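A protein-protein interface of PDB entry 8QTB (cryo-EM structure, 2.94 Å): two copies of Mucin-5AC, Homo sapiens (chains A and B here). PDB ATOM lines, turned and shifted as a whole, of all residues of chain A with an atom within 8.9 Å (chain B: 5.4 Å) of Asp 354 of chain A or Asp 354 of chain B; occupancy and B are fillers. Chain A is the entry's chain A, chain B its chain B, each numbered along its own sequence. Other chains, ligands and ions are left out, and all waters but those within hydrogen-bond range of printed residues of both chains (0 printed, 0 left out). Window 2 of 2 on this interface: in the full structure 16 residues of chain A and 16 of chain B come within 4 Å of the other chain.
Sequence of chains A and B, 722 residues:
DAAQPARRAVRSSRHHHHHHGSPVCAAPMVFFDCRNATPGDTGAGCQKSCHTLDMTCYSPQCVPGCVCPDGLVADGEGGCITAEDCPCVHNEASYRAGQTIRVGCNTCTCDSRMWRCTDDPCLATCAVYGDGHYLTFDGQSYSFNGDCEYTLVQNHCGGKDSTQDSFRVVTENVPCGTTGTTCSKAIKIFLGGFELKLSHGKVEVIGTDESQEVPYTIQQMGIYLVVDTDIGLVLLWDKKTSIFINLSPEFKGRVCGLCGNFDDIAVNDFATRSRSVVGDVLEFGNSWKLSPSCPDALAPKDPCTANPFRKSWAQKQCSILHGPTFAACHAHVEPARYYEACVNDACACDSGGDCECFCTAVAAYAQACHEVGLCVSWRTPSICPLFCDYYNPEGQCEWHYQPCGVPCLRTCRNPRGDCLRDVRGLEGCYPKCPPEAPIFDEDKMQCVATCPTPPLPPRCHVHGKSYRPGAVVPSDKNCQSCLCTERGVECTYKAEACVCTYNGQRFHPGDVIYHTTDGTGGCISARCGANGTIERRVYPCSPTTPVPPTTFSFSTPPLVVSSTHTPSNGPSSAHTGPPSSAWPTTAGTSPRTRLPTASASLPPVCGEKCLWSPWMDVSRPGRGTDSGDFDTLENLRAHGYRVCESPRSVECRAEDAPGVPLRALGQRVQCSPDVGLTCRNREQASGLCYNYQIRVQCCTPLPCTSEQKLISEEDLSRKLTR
NH1 of Arg 310 of chain B sits at hydrogen-bond distance from O of Asp 350 of chain A, at 3.2 Å. OD2 of Asp 354 of chain A sits at hydrogen-bond distance from N of Gly 353 of chain B. OD1 of Asp 354 of chain A lies close to OD1 of Asp 354 of chain B, at 2.9 Å. N of Gly 353 of chain A is in hydrogen-bond range of OD2 of Asp 354 of chain B.
The side-chain sulfur (SG) of Cys 318 of chain A is disulfide-bonded to the side-chain sulfur (SG) of Cys 342 of chain A, 2.0 Å away. The guanidinium group (NH2) of Arg 310 of chain A lies within salt-bridge range of the side-chain carboxylate (OD2) of Asp 354 of chain A, 3.6 Å away. The side-chain sulfur (SG) of Cys 384 of chain A forms a disulfide with the side-chain sulfur (SG) of Cys 359 of chain A, at 2.0 Å. NH2 of Arg 310 of chain B is in hydrogen-bond range of O of Ala 346 of chain B. NH2 of Arg 310 of chain B lies within hydrogen-bond range of O of Cys 349 of chain B (2.9 Å). The side-chain sulfur (SG) of Cys 357 of chain B forms a disulfide with the side-chain sulfur (SG) of Cys 349 of chain B (2.0 Å).
Among the printed residues, merely in contact across the chains: Trp 313 of chain A with Gly 352 of chain B, Trp 313 of chain A with Gly 353 of chain B, Gly 352 of chain A with Trp 313 of chain B, Gly 352 of chain A with Asp 354 of chain B, Gly 353 of chain A with Trp 313 of chain B and Asp 354 of chain A with Gly 352 of chain B.
Arg 310 of chain A touches none of the printed residues of chain B. Asp 345 of chain A touches none of the printed residues of chain B. Of the printed residues of chain B, Asp 350 of chain A touches Arg 310. Of the printed residues of chain B, Gly 353 of chain A touches Trp 313 and Asp 354. Asp 354 of chain A touches just these residues of chain B: Gly 352 (3.4 Å), Gly 353 (3.2 Å) and Asp 354 (2.9 Å). Of the printed residues of chain A, Arg 310 of chain B touches Asp 350. Of the printed residues of chain A, Trp 313 of chain B touches Gly 352 (3.98 Å) and Gly 353 (3.6 Å). Gly 353 of chain B touches just these residues of chain A: Trp 313 (3.7 Å) and Asp 354 (3.2 Å). Of the printed residues of chain A, Asp 354 of chain B touches Gly 352 (3.3 Å), Gly 353 (3.2 Å) and Asp 354 (2.9 Å). The nearest residue of chain A that does not touch Asp 354 of chain B is Cys 355 of chain A (5.0 Å). The nearest printed residue of chain A that does not touch Arg 310 of chain B is Gly 352 of chain A (4.2 Å).
Hydrophobic or aromatic side chains of chain B within 4 Å of the printed part of chain A: Trp 313. Among the printed residues, 10 pairs touch across the chains. Among the printed residues, no Asp or Glu carboxylate lies within 4 Å of a Lys or Arg side-chain nitrogen of the other chain.
Trp 313 of chain A touches Gly 352 of chain B, and with the chains exchanged Gly 352 of chain A touches Trp 313 of chain B. Trp 313 of chain A touches Gly 353 of chain B, and with the chains exchanged Gly 353 of chain A touches Trp 313 of chain B. Gly 352 of chain A touches Asp 354 of chain B, and with the chains exchanged Asp 354 of chain A touches Gly 352 of chain B. Gly 353 of chain A touches Asp 354 of chain B, and with the chains exchanged Asp 354 of chain A touches Gly 353 of chain B. 12 positions are printed for both chains.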
ATOM      1  N   ARG A 310       6.032 -28.851  23.265  1.00  0.00           N
ATOM      2  CA  ARG A 310       4.899 -28.081  22.773  1.00  0.00           C
ATOM      3  C   ARG A 310       3.608 -28.368  23.529  1.00  0.00           C
ATOM      4  O   ARG A 310       2.599 -27.698  23.278  1.00  0.00           O
ATOM      5  CB  ARG A 310       4.682 -28.356  21.280  1.00  0.00           C
ATOM      6  CG  ARG A 310       5.927 -28.180  20.430  1.00  0.00           C
ATOM      7  CD  ARG A 310       5.684 -28.627  18.998  1.00  0.00           C
ATOM      8  NE  ARG A 310       4.581 -27.901  18.381  1.00  0.00           N
ATOM      9  CZ  ARG A 310       4.712 -26.753  17.729  1.00  0.00           C
ATOM     10  NH1 ARG A 310       5.890 -26.168  17.591  1.00  0.00           N
ATOM     11  NH2 ARG A 310       3.634 -26.178  17.204  1.00  0.00           N
ATOM     12  N   TRP A 313       2.123 -25.289  25.698  1.00  0.00           N
ATOM     13  CA  TRP A 313       1.531 -24.255  24.856  1.00  0.00           C
ATOM     14  C   TRP A 313       0.259 -24.755  24.185  1.00  0.00           C
ATOM     15  O   TRP A 313      -0.729 -24.017  24.082  1.00  0.00           O
ATOM     16  CB  TRP A 313       2.544 -23.787  23.813  1.00  0.00           C
ATOM     17  CG  TRP A 313       2.055 -22.660  22.958  1.00  0.00           C
ATOM     18  CD1 TRP A 313       2.107 -21.329  23.249  1.00  0.00           C
ATOM     19  CD2 TRP A 313       1.441 -22.765  21.669  1.00  0.00           C
ATOM     20  NE1 TRP A 313       1.563 -20.598  22.222  1.00  0.00           N
ATOM     21  CE2 TRP A 313       1.147 -21.457  21.239  1.00  0.00           C
ATOM     22  CE3 TRP A 313       1.112 -23.839  20.837  1.00  0.00           C
ATOM     23  CZ2 TRP A 313       0.538 -21.193  20.014  1.00  0.00           C
ATOM     24  CZ3 TRP A 313       0.508 -23.574  19.621  1.00  0.00           C
ATOM     25  CH2 TRP A 313       0.227 -22.262  19.221  1.00  0.00           C
ATOM     26  N   ALA A 314       0.266 -26.006  23.720  1.00  0.00           N
ATOM     27  CA  ALA A 314      -0.917 -26.565  23.075  1.00  0.00           C
ATOM     28  C   ALA A 314      -2.098 -26.607  24.036  1.00  0.00           C
ATOM     29  O   ALA A 314      -3.219 -26.225  23.679  1.00  0.00           O
ATOM     30  CB  ALA A 314      -0.607 -27.961  22.539  1.00  0.00           C
ATOM     31  N   GLN A 317      -3.397 -23.060  24.769  1.00  0.00           N
ATOM     32  CA  GLN A 317      -4.171 -22.502  23.667  1.00  0.00           C
ATOM     33  C   GLN A 317      -5.529 -23.182  23.531  1.00  0.00           C
ATOM     34  O   GLN A 317      -6.547 -22.508  23.340  1.00  0.00           O
ATOM     35  CB  GLN A 317      -3.381 -22.612  22.364  1.00  0.00           C
ATOM     36  CG  GLN A 317      -2.186 -21.678  22.292  1.00  0.00           C
ATOM     37  CD  GLN A 317      -2.588 -20.218  22.277  1.00  0.00           C
ATOM     38  OE1 GLN A 317      -3.665 -19.863  21.798  1.00  0.00           O
ATOM     39  NE2 GLN A 317      -1.722 -19.360  22.803  1.00  0.00           N
ATOM     40  N   CYS A 318      -5.571 -24.512  23.634  1.00  0.00           N
ATOM     41  CA  CYS A 318      -6.820 -25.234  23.425  1.00  0.00           C
ATOM     42  C   CYS A 318      -7.724 -25.241  24.651  1.00  0.00           C
ATOM     43  O   CYS A 318      -8.850 -25.742  24.563  1.00  0.00           O
ATOM     44  CB  CYS A 318      -6.537 -26.678  22.995  1.00  0.00           C
ATOM     45  SG  CYS A 318      -5.655 -26.850  21.421  1.00  0.00           S
ATOM     46  N   CYS A 342      -7.881 -30.620  18.968  1.00  0.00           N
ATOM     47  CA  CYS A 342      -7.109 -29.384  19.050  1.00  0.00           C
ATOM     48  C   CYS A 342      -5.725 -29.647  19.627  1.00  0.00           C
ATOM     49  O   CYS A 342      -4.717 -29.159  19.102  1.00  0.00           O
ATOM     50  CB  CYS A 342      -7.856 -28.355  19.902  1.00  0.00           C
ATOM     51  SG  CYS A 342      -7.091 -26.709  19.987  1.00  0.00           S
ATOM     52  N   ASP A 345      -3.585 -31.633  17.059  1.00  0.00           N
ATOM     53  CA  ASP A 345      -3.189 -30.811  15.922  1.00  0.00           C
ATOM     54  C   ASP A 345      -2.133 -29.790  16.318  1.00  0.00           C
ATOM     55  O   ASP A 345      -1.165 -29.572  15.581  1.00  0.00           O
ATOM     56  CB  ASP A 345      -4.412 -30.118  15.323  1.00  0.00           C
ATOM     57  CG  ASP A 345      -5.218 -31.035  14.426  1.00  0.00           C
ATOM     58  OD1 ASP A 345      -4.964 -32.258  14.442  1.00  0.00           O
ATOM     59  OD2 ASP A 345      -6.103 -30.534  13.701  1.00  0.00           O
ATOM     60  N   ALA A 346      -2.293 -29.158  17.485  1.00  0.00           N
ATOM     61  CA  ALA A 346      -1.296 -28.195  17.938  1.00  0.00           C
ATOM     62  C   ALA A 346       0.040 -28.874  18.204  1.00  0.00           C
ATOM     63  O   ALA A 346       1.102 -28.302  17.929  1.00  0.00           O
ATOM     64  CB  ALA A 346      -1.793 -27.472  19.187  1.00  0.00           C
ATOM     65  N   CYS A 347       0.011 -30.095  18.745  1.00  0.00           N
ATOM     66  CA  CYS A 347       1.247 -30.842  18.944  1.00  0.00           C
ATOM     67  C   CYS A 347       1.907 -31.184  17.614  1.00  0.00           C
ATOM     68  O   CYS A 347       3.138 -31.130  17.492  1.00  0.00           O
ATOM     69  CB  CYS A 347       0.971 -32.112  19.749  1.00  0.00           C
ATOM     70  SG  CYS A 347       1.024 -31.895  21.546  1.00  0.00           S
ATOM     71  N   ALA A 348       1.109 -31.537  16.603  1.00  0.00           N
ATOM     72  CA  ALA A 348       1.665 -31.980  15.330  1.00  0.00           C
ATOM     73  C   ALA A 348       2.010 -30.822  14.400  1.00  0.00           C
ATOM     74  O   ALA A 348       2.873 -30.974  13.529  1.00  0.00           O
ATOM     75  CB  ALA A 348       0.690 -32.927  14.631  1.00  0.00           C
ATOM     76  N   CYS A 349       1.358 -29.670  14.561  1.00  0.00           N
ATOM     77  CA  CYS A 349       1.557 -28.531  13.663  1.00  0.00           C
ATOM     78  C   CYS A 349       2.857 -27.798  14.014  1.00  0.00           C
ATOM     79  O   CYS A 349       2.871 -26.630  14.401  1.00  0.00           O
ATOM     80  CB  CYS A 349       0.352 -27.600  13.730  1.00  0.00           C
ATOM     81  SG  CYS A 349       0.052 -26.585  12.260  1.00  0.00           S
ATOM     82  N   ASP A 350       3.969 -28.518  13.868  1.00  0.00           N
ATOM     83  CA  ASP A 350       5.283 -28.021  14.260  1.00  0.00           C
ATOM     84  C   ASP A 350       6.168 -27.664  13.072  1.00  0.00           C
ATOM     85  O   ASP A 350       7.372 -27.455  13.252  1.00  0.00           O
ATOM     86  CB  ASP A 350       5.993 -29.047  15.148  1.00  0.00           C
ATOM     87  CG  ASP A 350       6.303 -30.341  14.417  1.00  0.00           C
ATOM     88  OD1 ASP A 350       5.723 -30.578  13.337  1.00  0.00           O
ATOM     89  OD2 ASP A 350       7.132 -31.123  14.927  1.00  0.00           O
ATOM     90  N   SER A 351       5.610 -27.593  11.865  1.00  0.00           N
ATOM     91  CA  SER A 351       6.365 -27.225  10.676  1.00  0.00           C
ATOM     92  C   SER A 351       6.123 -25.779  10.261  1.00  0.00           C
ATOM     93  O   SER A 351       6.451 -25.400   9.133  1.00  0.00           O
ATOM     94  CB  SER A 351       6.028 -28.170   9.521  1.00  0.00           C
ATOM     95  OG  SER A 351       6.856 -27.915   8.401  1.00  0.00           O
ATOM     96  N   GLY A 352       5.561 -24.973  11.145  1.00  0.00           N
ATOM     97  CA  GLY A 352       5.237 -23.596  10.840  1.00  0.00           C
ATOM     98  C   GLY A 352       3.742 -23.389  10.685  1.00  0.00           C
ATOM     99  O   GLY A 352       3.007 -24.263  10.213  1.00  0.00           O
ATOM    100  N   GLY A 353       3.282 -22.208  11.085  1.00  0.00           N
ATOM    101  CA  GLY A 353       1.867 -21.892  11.013  1.00  0.00           C
ATOM    102  C   GLY A 353       0.991 -22.697  11.947  1.00  0.00           C
ATOM    103  O   GLY A 353      -0.106 -23.114  11.555  1.00  0.00           O
ATOM    104  N   ASP A 354       1.451 -22.933  13.179  1.00  0.00           N
ATOM    105  CA  ASP A 354       0.619 -23.620  14.163  1.00  0.00           C
ATOM    106  C   ASP A 354      -0.626 -22.814  14.498  1.00  0.00           C
ATOM    107  O   ASP A 354      -1.665 -23.387  14.861  1.00  0.00           O
ATOM    108  CB  ASP A 354       1.430 -23.903  15.428  1.00  0.00           C
ATOM    109  CG  ASP A 354       2.111 -22.663  15.971  1.00  0.00           C
ATOM    110  OD1 ASP A 354       2.060 -21.612  15.300  1.00  0.00           O
ATOM    111  OD2 ASP A 354       2.698 -22.740  17.071  1.00  0.00           O
ATOM    112  N   CYS A 355      -0.541 -21.486  14.389  1.00  0.00           N
ATOM    113  CA  CYS A 355      -1.711 -20.645  14.607  1.00  0.00           C
ATOM    114  C   CYS A 355      -2.823 -20.995  13.630  1.00  0.00           C
ATOM    115  O   CYS A 355      -4.003 -20.989  13.996  1.00  0.00           O
ATOM    116  CB  CYS A 355      -1.326 -19.170  14.481  1.00  0.00           C
ATOM    117  SG  CYS A 355      -2.726 -18.029  14.489  1.00  0.00           S
ATOM    118  N   GLU A 356      -2.468 -21.305  12.382  1.00  0.00           N
ATOM    119  CA  GLU A 356      -3.475 -21.719  11.411  1.00  0.00           C
ATOM    120  C   GLU A 356      -4.153 -23.016  11.835  1.00  0.00           C
ATOM    121  O   GLU A 356      -5.377 -23.146  11.724  1.00  0.00           O
ATOM    122  CB  GLU A 356      -2.845 -21.871  10.027  1.00  0.00           C
ATOM    123  CG  GLU A 356      -2.362 -20.567   9.419  1.00  0.00           C
ATOM    124  CD  GLU A 356      -2.190 -20.657   7.915  1.00  0.00           C
ATOM    125  OE1 GLU A 356      -2.570 -21.695   7.334  1.00  0.00           O
ATOM    126  OE2 GLU A 356      -1.676 -19.690   7.315  1.00  0.00           O
ATOM    127  N   CYS A 357      -3.376 -23.987  12.322  1.00  0.00           N
ATOM    128  CA  CYS A 357      -3.962 -25.243  12.783  1.00  0.00           C
ATOM    129  C   CYS A 357      -4.920 -25.010  13.946  1.00  0.00           C
ATOM    130  O   CYS A 357      -6.043 -25.539  13.961  1.00  0.00           O
ATOM    131  CB  CYS A 357      -2.851 -26.217  13.184  1.00  0.00           C
ATOM    132  SG  CYS A 357      -1.904 -26.912  11.798  1.00  0.00           S
ATOM    133  N   PHE A 358      -4.498 -24.203  14.924  1.00  0.00           N
ATOM    134  CA  PHE A 358      -5.350 -23.918  16.073  1.00  0.00           C
ATOM    135  C   PHE A 358      -6.626 -23.195  15.653  1.00  0.00           C
ATOM    136  O   PHE A 358      -7.725 -23.535  16.115  1.00  0.00           O
ATOM    137  CB  PHE A 358      -4.571 -23.092  17.097  1.00  0.00           C
ATOM    138  CG  PHE A 358      -5.421 -22.521  18.195  1.00  0.00           C
ATOM    139  CD1 PHE A 358      -5.929 -23.337  19.191  1.00  0.00           C
ATOM    140  CD2 PHE A 358      -5.704 -21.167  18.234  1.00  0.00           C
ATOM    141  CE1 PHE A 358      -6.706 -22.813  20.203  1.00  0.00           C
ATOM    142  CE2 PHE A 358      -6.483 -20.637  19.244  1.00  0.00           C
ATOM    143  CZ  PHE A 358      -6.984 -21.462  20.229  1.00  0.00           C
ATOM    144  N   CYS A 359      -6.497 -22.198  14.773  1.00  0.00           N
ATOM    145  CA  CYS A 359      -7.664 -21.457  14.311  1.00  0.00           C
ATOM    146  C   CYS A 359      -8.616 -22.357  13.538  1.00  0.00           C
ATOM    147  O   CYS A 359      -9.836 -22.236  13.676  1.00  0.00           O
ATOM    148  CB  CYS A 359      -7.229 -20.270  13.452  1.00  0.00           C
ATOM    149  SG  CYS A 359      -6.406 -18.932  14.354  1.00  0.00           S
ATOM    150  N   THR A 360      -8.081 -23.260  12.712  1.00  0.00           N
ATOM    151  CA  THR A 360      -8.942 -24.177  11.972  1.00  0.00           C
ATOM    152  C   THR A 360      -9.703 -25.100  12.913  1.00  0.00           C
ATOM    153  O   THR A 360     -10.899 -25.341  12.719  1.00  0.00           O
ATOM    154  CB  THR A 360      -8.120 -24.995  10.976  1.00  0.00           C
ATOM    155  OG1 THR A 360      -6.928 -25.470  11.611  1.00  0.00           O
ATOM    156  CG2 THR A 360      -7.746 -24.147   9.768  1.00  0.00           C
ATOM    157  N   ALA A 361      -9.030 -25.626  13.940  1.00  0.00           N
ATOM    158  CA  ALA A 361      -9.726 -26.489  14.893  1.00  0.00           C
ATOM    159  C   ALA A 361     -10.828 -25.731  15.628  1.00  0.00           C
ATOM    160  O   ALA A 361     -11.960 -26.226  15.763  1.00  0.00           O
ATOM    161  CB  ALA A 361      -8.730 -27.086  15.886  1.00  0.00           C
ATOM    162  N   CYS A 384      -6.981 -15.557  16.885  1.00  0.00           N
ATOM    163  CA  CYS A 384      -7.496 -15.730  15.529  1.00  0.00           C
ATOM    164  C   CYS A 384      -8.232 -14.481  15.054  1.00  0.00           C
ATOM    165  O   CYS A 384      -9.450 -14.527  14.837  1.00  0.00           O
ATOM    166  CB  CYS A 384      -8.423 -16.946  15.460  1.00  0.00           C
ATOM    167  SG  CYS A 384      -7.649 -18.519  15.907  1.00  0.00           S
ATOM    168  N   ARG B 310      12.369 -26.217   9.191  1.00  0.00           N
ATOM    169  CA  ARG B 310      11.670 -24.940   9.245  1.00  0.00           C
ATOM    170  C   ARG B 310      12.276 -23.889   8.324  1.00  0.00           C
ATOM    171  O   ARG B 310      11.708 -22.798   8.197  1.00  0.00           O
ATOM    172  CB  ARG B 310      11.656 -24.406  10.681  1.00  0.00           C
ATOM    173  CG  ARG B 310      11.146 -25.400  11.709  1.00  0.00           C
ATOM    174  CD  ARG B 310      11.313 -24.868  13.122  1.00  0.00           C
ATOM    175  NE  ARG B 310      10.628 -23.595  13.311  1.00  0.00           N
ATOM    176  CZ  ARG B 310       9.364 -23.476  13.691  1.00  0.00           C
ATOM    177  NH1 ARG B 310       8.612 -24.538  13.933  1.00  0.00           N
ATOM    178  NH2 ARG B 310       8.840 -22.262  13.832  1.00  0.00           N
ATOM    179  N   TRP B 313       9.937 -22.702   5.240  1.00  0.00           N
ATOM    180  CA  TRP B 313       8.839 -21.847   5.677  1.00  0.00           C
ATOM    181  C   TRP B 313       9.352 -20.500   6.165  1.00  0.00           C
ATOM    182  O   TRP B 313       8.747 -19.456   5.886  1.00  0.00           O
ATOM    183  CB  TRP B 313       8.035 -22.547   6.772  1.00  0.00           C
ATOM    184  CG  TRP B 313       6.830 -21.781   7.220  1.00  0.00           C
ATOM    185  CD1 TRP B 313       5.593 -21.790   6.647  1.00  0.00           C
ATOM    186  CD2 TRP B 313       6.746 -20.895   8.342  1.00  0.00           C
ATOM    187  NE1 TRP B 313       4.744 -20.963   7.341  1.00  0.00           N
ATOM    188  CE2 TRP B 313       5.427 -20.402   8.387  1.00  0.00           C
ATOM    189  CE3 TRP B 313       7.658 -20.470   9.313  1.00  0.00           C
ATOM    190  CZ2 TRP B 313       4.998 -19.505   9.362  1.00  0.00           C
ATOM    191  CZ3 TRP B 313       7.229 -19.580  10.281  1.00  0.00           C
ATOM    192  CH2 TRP B 313       5.912 -19.107  10.298  1.00  0.00           C
ATOM    193  N   ALA B 346      12.569 -16.828  13.020  1.00  0.00           N
ATOM    194  CA  ALA B 346      11.599 -17.822  12.574  1.00  0.00           C
ATOM    195  C   ALA B 346      12.136 -19.235  12.757  1.00  0.00           C
ATOM    196  O   ALA B 346      11.384 -20.152  13.107  1.00  0.00           O
ATOM    197  CB  ALA B 346      11.221 -17.570  11.115  1.00  0.00           C
ATOM    198  N   CYS B 349      11.977 -19.729  16.678  1.00  0.00           N
ATOM    199  CA  CYS B 349      10.661 -19.620  17.309  1.00  0.00           C
ATOM    200  C   CYS B 349       9.851 -20.900  17.076  1.00  0.00           C
ATOM    201  O   CYS B 349       8.798 -20.907  16.441  1.00  0.00           O
ATOM    202  CB  CYS B 349       9.932 -18.391  16.778  1.00  0.00           C
ATOM    203  SG  CYS B 349       8.684 -17.673  17.876  1.00  0.00           S
ATOM    204  N   GLY B 352       6.162 -22.620  19.712  1.00  0.00           N
ATOM    205  CA  GLY B 352       4.807 -22.121  19.616  1.00  0.00           C
ATOM    206  C   GLY B 352       4.770 -20.619  19.403  1.00  0.00           C
ATOM    207  O   GLY B 352       5.617 -19.868  19.901  1.00  0.00           O
ATOM    208  N   GLY B 353       3.770 -20.170  18.654  1.00  0.00           N
ATOM    209  CA  GLY B 353       3.635 -18.755  18.355  1.00  0.00           C
ATOM    210  C   GLY B 353       4.725 -18.191  17.471  1.00  0.00           C
ATOM    211  O   GLY B 353       5.194 -17.070  17.711  1.00  0.00           O
ATOM    212  N   ASP B 354       5.148 -18.943  16.450  1.00  0.00           N
ATOM    213  CA  ASP B 354       6.128 -18.421  15.502  1.00  0.00           C
ATOM    214  C   ASP B 354       5.581 -17.226  14.735  1.00  0.00           C
ATOM    215  O   ASP B 354       6.349 -16.352  14.308  1.00  0.00           O
ATOM    216  CB  ASP B 354       6.558 -19.525  14.534  1.00  0.00           C
ATOM    217  CG  ASP B 354       5.379 -20.209  13.872  1.00  0.00           C
ATOM    218  OD1 ASP B 354       4.227 -19.918  14.257  1.00  0.00           O
ATOM    219  OD2 ASP B 354       5.603 -21.041  12.968  1.00  0.00           O
ATOM    220  N   CYS B 355       4.260 -17.175  14.550  1.00  0.00           N
ATOM    221  CA  CYS B 355       3.644 -16.023  13.904  1.00  0.00           C
ATOM    222  C   CYS B 355       3.928 -14.745  14.682  1.00  0.00           C
ATOM    223  O   CYS B 355       4.155 -13.687  14.086  1.00  0.00           O
ATOM    224  CB  CYS B 355       2.139 -16.244  13.762  1.00  0.00           C
ATOM    225  SG  CYS B 355       1.219 -14.795  13.199  1.00  0.00           S
ATOM    226  N   GLU B 356       3.924 -14.826  16.014  1.00  0.00           N
ATOM    227  CA  GLU B 356       4.256 -13.657  16.823  1.00  0.00           C
ATOM    228  C   GLU B 356       5.691 -13.206  16.578  1.00  0.00           C
ATOM    229  O   GLU B 356       5.957 -12.005  16.458  1.00  0.00           O
ATOM    230  CB  GLU B 356       4.034 -13.958  18.304  1.00  0.00           C
ATOM    231  CG  GLU B 356       2.581 -14.176  18.681  1.00  0.00           C
ATOM    232  CD  GLU B 356       2.333 -14.001  20.165  1.00  0.00           C
ATOM    233  OE1 GLU B 356       3.269 -13.584  20.879  1.00  0.00           O
ATOM    234  OE2 GLU B 356       1.203 -14.280  20.619  1.00  0.00           O
ATOM    235  N   CYS B 357       6.631 -14.152  16.501  1.00  0.00           N
ATOM    236  CA  CYS B 357       8.021 -13.795  16.233  1.00  0.00           C
ATOM    237  C   CYS B 357       8.163 -13.118  14.873  1.00  0.00           C
ATOM    238  O   CYS B 357       8.828 -12.077  14.748  1.00  0.00           O
ATOM    239  CB  CYS B 357       8.902 -15.045  16.309  1.00  0.00           C
ATOM    240  SG  CYS B 357       9.163 -15.698  17.984  1.00  0.00           S
ATOM    241  N   PHE B 358       7.527 -13.688  13.846  1.00  0.00           N
ATOM    242  CA  PHE B 358       7.602 -13.107  12.509  1.00  0.00           C
ATOM    243  C   PHE B 358       6.983 -11.713  12.476  1.00  0.00           C
ATOM    244  O   PHE B 358       7.552 -10.783  11.887  1.00  0.00           O
ATOM    245  CB  PHE B 358       6.910 -14.031  11.508  1.00  0.00           C
ATOM    246  CG  PHE B 358       6.697 -13.416  10.157  1.00  0.00           C
ATOM    247  CD1 PHE B 358       7.761 -13.224   9.293  1.00  0.00           C
ATOM    248  CD2 PHE B 358       5.429 -13.039   9.746  1.00  0.00           C
ATOM    249  CE1 PHE B 358       7.566 -12.662   8.047  1.00  0.00           C
ATOM    250  CE2 PHE B 358       5.229 -12.476   8.501  1.00  0.00           C
ATOM    251  CZ  PHE B 358       6.298 -12.288   7.651  1.00  0.00           C
ATOM    252  N   CYS B 359       5.818 -11.551  13.107  1.00  0.00           N
ATOM    253  CA  CYS B 359       5.158 -10.251  13.132  1.00  0.00           C
ATOM    254  C   CYS B 359       5.995  -9.223  13.877  1.00  0.00           C
ATOM    255  O   CYS B 359       6.069  -8.062  13.463  1.00  0.00           O
ATOM    256  CB  CYS B 359       3.771 -10.375  13.764  1.00  0.00           C
ATOM    257  SG  CYS B 359       2.553 -11.272  12.768  1.00  0.00           S
